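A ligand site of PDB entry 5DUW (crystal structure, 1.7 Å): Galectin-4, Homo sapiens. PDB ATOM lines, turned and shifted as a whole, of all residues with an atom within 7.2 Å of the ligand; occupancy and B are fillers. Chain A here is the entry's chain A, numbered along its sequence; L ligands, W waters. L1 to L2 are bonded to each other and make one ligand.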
ATOM      1  N   ARG A  45      -1.029  28.955   1.196  1.00  0.00           N
ATOM      2  CA  ARG A  45      -2.114  28.681   0.224  1.00  0.00           C
ATOM      3  C   ARG A  45      -2.868  29.970  -0.071  1.00  0.00           C
ATOM      4  O   ARG A  45      -2.825  30.920   0.704  1.00  0.00           O
ATOM      5  CB  ARG A  45      -3.151  27.663   0.767  1.00  0.00           C
ATOM      6  CG  ARG A  45      -2.627  26.291   1.195  1.00  0.00           C
ATOM      7  CD  ARG A  45      -3.742  25.311   1.599  1.00  0.00           C
ATOM      8  NE  ARG A  45      -3.229  23.975   1.914  1.00  0.00           N
ATOM      9  CZ  ARG A  45      -3.956  22.948   2.307  1.00  0.00           C
ATOM     10  NH1 ARG A  45      -5.263  23.074   2.444  1.00  0.00           N
ATOM     11  NH2 ARG A  45      -3.380  21.782   2.574  1.00  0.00           N
ATOM     12  N   PHE A  47      -6.896  30.763  -2.260  1.00  0.00           N
ATOM     13  CA  PHE A  47      -7.913  30.216  -3.134  1.00  0.00           C
ATOM     14  C   PHE A  47      -8.725  31.297  -3.831  1.00  0.00           C
ATOM     15  O   PHE A  47      -8.821  32.444  -3.364  1.00  0.00           O
ATOM     16  CB  PHE A  47      -8.819  29.229  -2.411  1.00  0.00           C
ATOM     17  CG  PHE A  47      -9.611  29.832  -1.291  1.00  0.00           C
ATOM     18  CD1 PHE A  47     -10.737  30.571  -1.557  1.00  0.00           C
ATOM     19  CD2 PHE A  47      -9.206  29.667   0.023  1.00  0.00           C
ATOM     20  CE1 PHE A  47     -11.456  31.134  -0.539  1.00  0.00           C
ATOM     21  CE2 PHE A  47      -9.949  30.214   1.053  1.00  0.00           C
ATOM     22  CZ  PHE A  47     -11.076  30.952   0.777  1.00  0.00           C
ATOM     23  N   ASN A  49     -12.610  31.197  -5.324  1.00  0.00           N
ATOM     24  CA  ASN A  49     -13.867  30.441  -5.411  1.00  0.00           C
ATOM     25  C   ASN A  49     -14.901  31.170  -6.266  1.00  0.00           C
ATOM     26  O   ASN A  49     -15.109  32.375  -6.128  1.00  0.00           O
ATOM     27  CB  ASN A  49     -14.469  30.259  -4.019  1.00  0.00           C
ATOM     28  CG  ASN A  49     -13.734  29.254  -3.152  1.00  0.00           C
ATOM     29  OD1 ASN A  49     -12.969  28.419  -3.639  1.00  0.00           O
ATOM     30  ND2 ASN A  49     -13.993  29.302  -1.852  1.00  0.00           N
ATOM     31  N   VAL A  60     -19.730  26.010  -3.810  1.00  0.00           N
ATOM     32  CA  VAL A  60     -18.654  26.569  -4.600  1.00  0.00           C
ATOM     33  C   VAL A  60     -18.555  25.786  -5.891  1.00  0.00           C
ATOM     34  O   VAL A  60     -18.160  24.612  -5.893  1.00  0.00           O
ATOM     35  CB  VAL A  60     -17.329  26.524  -3.840  1.00  0.00           C
ATOM     36  CG1 VAL A  60     -16.195  27.033  -4.720  1.00  0.00           C
ATOM     37  CG2 VAL A  60     -17.408  27.297  -2.529  1.00  0.00           C
ATOM     38  N   HIS A  63     -13.443  25.853  -7.030  1.00  0.00           N
ATOM     39  CA  HIS A  63     -12.419  26.206  -6.051  1.00  0.00           C
ATOM     40  C   HIS A  63     -11.066  25.948  -6.713  1.00  0.00           C
ATOM     41  O   HIS A  63     -10.796  24.831  -7.154  1.00  0.00           O
ATOM     42  CB  HIS A  63     -12.600  25.278  -4.838  1.00  0.00           C
ATOM     43  CG  HIS A  63     -11.545  25.356  -3.778  1.00  0.00           C
ATOM     44  ND1 HIS A  63     -11.480  26.374  -2.849  1.00  0.00           N
ATOM     45  CD2 HIS A  63     -10.625  24.440  -3.383  1.00  0.00           C
ATOM     46  CE1 HIS A  63     -10.516  26.112  -1.977  1.00  0.00           C
ATOM     47  NE2 HIS A  63      -9.999  24.935  -2.268  1.00  0.00           N
ATOM     48  N   ASN A  65      -7.083  26.358  -5.945  1.00  0.00           N
ATOM     49  CA  ASN A  65      -6.369  26.391  -4.668  1.00  0.00           C
ATOM     50  C   ASN A  65      -4.881  26.001  -4.805  1.00  0.00           C
ATOM     51  O   ASN A  65      -4.523  24.846  -4.615  1.00  0.00           O
ATOM     52  CB  ASN A  65      -7.094  25.447  -3.709  1.00  0.00           C
ATOM     53  CG  ASN A  65      -6.518  25.384  -2.304  1.00  0.00           C
ATOM     54  OD1 ASN A  65      -6.607  24.337  -1.671  1.00  0.00           O
ATOM     55  ND2 ASN A  65      -5.993  26.504  -1.786  1.00  0.00           N
ATOM     56  N   ARG A  67      -1.247  25.457  -3.485  1.00  0.00           N
ATOM     57  CA  ARG A  67      -0.705  25.034  -2.200  1.00  0.00           C
ATOM     58  C   ARG A  67       0.830  24.833  -2.225  1.00  0.00           C
ATOM     59  O   ARG A  67       1.332  24.148  -3.108  1.00  0.00           O
ATOM     60  CB  ARG A  67      -1.321  23.722  -1.802  1.00  0.00           C
ATOM     61  CG  ARG A  67      -2.826  23.756  -1.624  1.00  0.00           C
ATOM     62  CD  ARG A  67      -3.326  22.402  -1.180  1.00  0.00           C
ATOM     63  NE  ARG A  67      -4.773  22.367  -0.991  1.00  0.00           N
ATOM     64  CZ  ARG A  67      -5.452  21.300  -0.608  1.00  0.00           C
ATOM     65  NH1 ARG A  67      -4.834  20.160  -0.356  1.00  0.00           N
ATOM     66  NH2 ARG A  67      -6.768  21.384  -0.477  1.00  0.00           N
ATOM     67  N   VAL A  75      -4.892  22.539  -6.416  1.00  0.00           N
ATOM     68  CA  VAL A  75      -6.048  21.691  -6.261  1.00  0.00           C
ATOM     69  C   VAL A  75      -7.263  22.397  -6.840  1.00  0.00           C
ATOM     70  O   VAL A  75      -7.400  23.624  -6.699  1.00  0.00           O
ATOM     71  CB  VAL A  75      -6.263  21.369  -4.773  1.00  0.00           C
ATOM     72  CG1 VAL A  75      -7.568  20.630  -4.566  1.00  0.00           C
ATOM     73  CG2 VAL A  75      -5.082  20.556  -4.243  1.00  0.00           C
ATOM     74  N   PHE A  76      -8.110  21.622  -7.506  1.00  0.00           N
ATOM     75  CA  PHE A  76      -9.327  22.098  -8.147  1.00  0.00           C
ATOM     76  C   PHE A  76     -10.478  21.230  -7.648  1.00  0.00           C
ATOM     77  O   PHE A  76     -10.385  20.003  -7.666  1.00  0.00           O
ATOM     78  CB  PHE A  76      -9.287  21.959  -9.677  1.00  0.00           C
ATOM     79  CG  PHE A  76      -8.015  22.447 -10.313  1.00  0.00           C
ATOM     80  CD1 PHE A  76      -6.926  21.622 -10.420  1.00  0.00           C
ATOM     81  CD2 PHE A  76      -7.926  23.735 -10.845  1.00  0.00           C
ATOM     82  CE1 PHE A  76      -5.744  22.053 -11.015  1.00  0.00           C
ATOM     83  CE2 PHE A  76      -6.751  24.174 -11.451  1.00  0.00           C
ATOM     84  CZ  PHE A  76      -5.656  23.330 -11.516  1.00  0.00           C
ATOM     85  N   ASN A  77     -11.576  21.847  -7.223  1.00  0.00           N
ATOM     86  CA  ASN A  77     -12.701  21.067  -6.734  1.00  0.00           C
ATOM     87  C   ASN A  77     -13.992  21.888  -6.734  1.00  0.00           C
ATOM     88  O   ASN A  77     -14.017  23.075  -7.069  1.00  0.00           O
ATOM     89  CB  ASN A  77     -12.383  20.515  -5.323  1.00  0.00           C
ATOM     90  CG  ASN A  77     -13.091  19.201  -5.009  1.00  0.00           C
ATOM     91  OD1 ASN A  77     -13.938  18.709  -5.758  1.00  0.00           O
ATOM     92  ND2 ASN A  77     -12.750  18.618  -3.869  1.00  0.00           N
ATOM     93  N   THR A  78     -15.054  21.218  -6.328  1.00  0.00           N
ATOM     94  CA  THR A  78     -16.378  21.797  -6.196  1.00  0.00           C
ATOM     95  C   THR A  78     -16.926  21.400  -4.811  1.00  0.00           C
ATOM     96  O   THR A  78     -16.778  20.261  -4.387  1.00  0.00           O
ATOM     97  CB  THR A  78     -17.283  21.254  -7.309  1.00  0.00           C
ATOM     98  OG1 THR A  78     -16.850  21.760  -8.575  1.00  0.00           O
ATOM     99  CG2 THR A  78     -18.738  21.608  -7.090  1.00  0.00           C
ATOM    100  N   LEU A  79     -17.568  22.356  -4.141  1.00  0.00           N
ATOM    101  CA  LEU A  79     -18.251  22.129  -2.871  1.00  0.00           C
ATOM    102  C   LEU A  79     -19.748  22.212  -3.160  1.00  0.00           C
ATOM    103  O   LEU A  79     -20.246  23.243  -3.603  1.00  0.00           O
ATOM    104  CB  LEU A  79     -17.874  23.198  -1.856  1.00  0.00           C
ATOM    105  CG  LEU A  79     -18.556  23.083  -0.474  1.00  0.00           C
ATOM    106  CD1 LEU A  79     -17.976  21.915   0.315  1.00  0.00           C
ATOM    107  CD2 LEU A  79     -18.366  24.378   0.293  1.00  0.00           C
ATOM    108  N   TRP A  84     -17.199  18.391  -0.317  1.00  0.00           N
ATOM    109  CA  TRP A  84     -16.171  18.516  -1.351  1.00  0.00           C
ATOM    110  C   TRP A  84     -16.194  17.288  -2.246  1.00  0.00           C
ATOM    111  O   TRP A  84     -16.376  16.152  -1.770  1.00  0.00           O
ATOM    112  CB  TRP A  84     -14.775  18.702  -0.755  1.00  0.00           C
ATOM    113  CG  TRP A  84     -14.512  20.048  -0.207  1.00  0.00           C
ATOM    114  CD1 TRP A  84     -14.395  20.387   1.105  1.00  0.00           C
ATOM    115  CD2 TRP A  84     -14.390  21.266  -0.947  1.00  0.00           C
ATOM    116  NE1 TRP A  84     -14.166  21.707   1.225  1.00  0.00           N
ATOM    117  CE2 TRP A  84     -14.171  22.289  -0.008  1.00  0.00           C
ATOM    118  CE3 TRP A  84     -14.414  21.592  -2.309  1.00  0.00           C
ATOM    119  CZ2 TRP A  84     -13.987  23.608  -0.388  1.00  0.00           C
ATOM    120  CZ3 TRP A  84     -14.244  22.915  -2.688  1.00  0.00           C
ATOM    121  CH2 TRP A  84     -14.029  23.912  -1.717  1.00  0.00           C
ATOM    122  N   GLY A  85     -16.044  17.503  -3.550  1.00  0.00           N
ATOM    123  CA  GLY A  85     -16.051  16.426  -4.508  1.00  0.00           C
ATOM    124  C   GLY A  85     -14.696  15.760  -4.635  1.00  0.00           C
ATOM    125  O   GLY A  85     -13.832  15.934  -3.761  1.00  0.00           O
ATOM    126  N   SER A  86     -14.518  14.989  -5.701  1.00  0.00           N
ATOM    127  CA  SER A  86     -13.226  14.407  -6.011  1.00  0.00           C
ATOM    128  C   SER A  86     -12.291  15.454  -6.560  1.00  0.00           C
ATOM    129  O   SER A  86     -12.586  16.083  -7.566  1.00  0.00           O
ATOM    130  CB  SER A  86     -13.365  13.265  -7.026  1.00  0.00           C
ATOM    131  OG  SER A  86     -14.150  12.243  -6.489  1.00  0.00           O
ATOM    132  N   GLU A  87     -11.170  15.656  -5.886  1.00  0.00           N
ATOM    133  CA  GLU A  87     -10.230  16.701  -6.294  1.00  0.00           C
ATOM    134  C   GLU A  87      -9.590  16.374  -7.608  1.00  0.00           C
ATOM    135  O   GLU A  87      -9.294  15.208  -7.895  1.00  0.00           O
ATOM    136  CB  GLU A  87      -9.104  16.847  -5.275  1.00  0.00           C
ATOM    137  CG  GLU A  87      -9.541  17.447  -3.987  1.00  0.00           C
ATOM    138  CD  GLU A  87      -8.409  17.560  -2.996  1.00  0.00           C
ATOM    139  OE1 GLU A  87      -8.634  18.263  -1.992  1.00  0.00           O
ATOM    140  OE2 GLU A  87      -7.284  17.027  -3.239  1.00  0.00           O
ATOM    141  N   GLU A  88      -9.390  17.402  -8.418  1.00  0.00           N
ATOM    142  CA  GLU A  88      -8.445  17.328  -9.510  1.00  0.00           C
ATOM    143  C   GLU A  88      -7.200  18.067  -9.009  1.00  0.00           C
ATOM    144  O   GLU A  88      -7.309  18.981  -8.201  1.00  0.00           O
ATOM    145  CB  GLU A  88      -9.019  17.933 -10.778  1.00  0.00           C
ATOM    146  CG  GLU A  88     -10.191  17.132 -11.309  1.00  0.00           C
ATOM    147  CD  GLU A  88     -10.960  17.809 -12.418  1.00  0.00           C
ATOM    148  OE1 GLU A  88     -10.332  18.395 -13.322  1.00  0.00           O
ATOM    149  OE2 GLU A  88     -12.202  17.697 -12.427  1.00  0.00           O
ATOM    150  N   ARG A  89      -6.032  17.649  -9.475  1.00  0.00           N
ATOM    151  CA  ARG A  89      -4.790  18.219  -9.010  1.00  0.00           C
ATOM    152  C   ARG A  89      -3.826  18.346 -10.160  1.00  0.00           C
ATOM    153  O   ARG A  89      -3.776  17.476 -11.029  1.00  0.00           O
ATOM    154  CB  ARG A  89      -4.162  17.318  -7.974  1.00  0.00           C
ATOM    155  CG  ARG A  89      -4.987  17.141  -6.728  1.00  0.00           C
ATOM    156  CD  ARG A  89      -4.288  16.237  -5.717  1.00  0.00           C
ATOM    157  NE  ARG A  89      -5.226  15.825  -4.676  1.00  0.00           N
ATOM    158  CZ  ARG A  89      -5.272  14.627  -4.094  1.00  0.00           C
ATOM    159  NH1 ARG A  89      -4.419  13.664  -4.425  1.00  0.00           N
ATOM    160  NH2 ARG A  89      -6.194  14.376  -3.158  1.00  0.00           N
HETATM  161  C1  LIG L   1      -7.340  16.259   0.708  1.00  0.00           C
HETATM  162  C2  LIG L   1      -7.420  17.734   1.067  1.00  0.00           C
HETATM  163  C3  LIG L   1      -8.819  18.121   1.531  1.00  0.00           C
HETATM  164  C4  LIG L   1      -9.299  17.149   2.606  1.00  0.00           C
HETATM  165  C5  LIG L   1     -10.709  17.447   3.098  1.00  0.00           C
HETATM  166  C6  LIG L   1      -7.913  15.407   1.840  1.00  0.00           C
HETATM  167  O1  LIG L   1      -7.913  14.055   1.366  1.00  0.00           O
HETATM  168  O2  LIG L   1      -5.962  15.913   0.483  1.00  0.00           O
HETATM  169  O3  LIG L   1      -7.017  18.499  -0.057  1.00  0.00           O
HETATM  170  O4  LIG L   1      -8.714  19.448   2.050  1.00  0.00           O
HETATM  171  O5  LIG L   1      -9.254  15.813   2.098  1.00  0.00           O
HETATM  172  O6  LIG L   1     -11.660  17.413   2.038  1.00  0.00           O
HETATM  173  C1  LG2 L   2      -9.731  20.309   1.556  1.00  0.00           C
HETATM  174  C2  LG2 L   2      -9.492  21.644   2.237  1.00  0.00           C
HETATM  175  C3  LG2 L   2     -10.373  22.745   1.674  1.00  0.00           C
HETATM  176  C4  LG2 L   2     -10.347  22.740   0.144  1.00  0.00           C
HETATM  177  C5  LG2 L   2     -10.598  21.319  -0.398  1.00  0.00           C
HETATM  178  C6  LG2 L   2     -10.501  21.205  -1.914  1.00  0.00           C
HETATM  179  O1  LG2 L   2      -9.785  21.484   3.636  1.00  0.00           O
HETATM  180  O2  LG2 L   2      -9.882  23.975   2.195  1.00  0.00           O
HETATM  181  O3  LG2 L   2      -9.045  23.184  -0.270  1.00  0.00           O
HETATM  182  O4  LG2 L   2      -9.615  20.426   0.141  1.00  0.00           O
HETATM  183  O5  LG2 L   2     -10.697  19.836  -2.323  1.00  0.00           O
HETATM  184  S1  LG2 L   2     -10.918  25.139   2.482  1.00  0.00           S
HETATM  185  O6  LG2 L   2     -11.853  25.387   1.368  1.00  0.00           O
HETATM  186  O7  LG2 L   2     -10.088  26.353   2.751  1.00  0.00           O
HETATM  187  O8  LG2 L   2     -11.552  24.716   3.704  1.00  0.00           O
HETATM  188  O   HOH W   1      -4.246  13.834   0.286  1.00  0.00           O
HETATM  189  O   HOH W   2     -13.838  23.417   3.679  1.00  0.00           O
HETATM  190  O   HOH W   3      -4.866  17.110  -1.727  1.00  0.00           O
HETATM  191  O   HOH W   4      -7.272  25.301   1.473  1.00  0.00           O
HETATM  192  O   HOH W   5      -9.047  28.428   4.244  1.00  0.00           O
HETATM  193  O   HOH W   6     -12.491  27.846   0.126  1.00  0.00           O
HETATM  194  O   HOH W   7     -12.305  20.674   4.181  1.00  0.00           O
HETATM  195  O   HOH W   8     -13.818  16.317   2.380  1.00  0.00           O
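OE1 of Glu 87 lies within hydrogen-bond range of O3 of LIG L1, 2.5 Å away. The side-chain amide nitrogen (ND2) of Asn 77 lies within hydrogen-bond range of an oxygen (O5) of LG2 L2 (2.8 Å). The side-chain amide oxygen of Asn 65 sits at hydrogen-bond distance from an oxygen (O3) of LG2 L2 (3.0 Å). The guanidinium group (NH1) of Arg 67 lies within hydrogen-bond range of an oxygen (O3) of LIG L1, 2.8 Å away. NE2 of His 63 is in hydrogen-bond range of O3 of LG2 L2 (2.8 Å).
The backbone carbonyl oxygen (O) of Ser 86 lies close to the side-chain amide oxygen (OD1) of Asn 77 (3.5 Å). The backbone carbonyl oxygen of Gly 85 lies within hydrogen-bond range of the side-chain amide nitrogen of Asn 77 (2.9 Å). A ring nitrogen (NE2) of His 63 sits close to the side-chain amide oxygen (OD1) of Asn 65 (3.5 Å). The backbone NH of His 63 sits at hydrogen-bond distance from the backbone carbonyl oxygen of Asn 77. The backbone NH of Asn 65 sits at hydrogen-bond distance from the backbone carbonyl oxygen of Val 75 (2.9 Å). The side-chain carboxylate (OE1) of Glu 87 lies within salt-bridge range of the guanidinium group (NH2) of Arg 67 (3.9 Å). NE of Arg 67 sits at hydrogen-bond distance from OD1 of Asn 65 (2.8 Å). A ring nitrogen (ND1) of His 63 is in hydrogen-bond range of the side-chain amide oxygen (OD1) of Asn 49 (2.7 Å).
Merely in contact with the ligand: Trp 84, Val 75 and Arg 89. Hydrophobic or aromatic side chains that line the ligand: His 63, Val 75 and Trp 84. Eight residues have an atom within 4 Å of the ligand: His 63, Asn 65, Arg 67, Val 75, Asn 77, Trp 84, Glu 87 and Arg 89. The nearest printed residue that does not touch the ligand is Phe 47 (4.2 Å).
Water W2 lies within hydrogen-bond range of O8 of LG2 L2 (2.6 Å) and NE1 of Trp 84 (3.0 Å). Water W3 lies within hydrogen-bond range of an oxygen (O2) of LIG L1, the side-chain carboxylate of Glu 87, the guanidinium group of Arg 89 and the guanidinium group of Arg 67. Water W6 lies within hydrogen-bond range of O6 of LG2 L2 (2.8 Å), ND2 of Asn 49 (2.9 Å) and ND1 of His 63 (3.5 Å). Water W4 lies within hydrogen-bond range of an oxygen (O2) of LG2 L2 (3.0 Å), the guanidinium group of Arg 45 (3.2 Å) and the side-chain amide oxygen of Asn 65 (3.4 Å).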
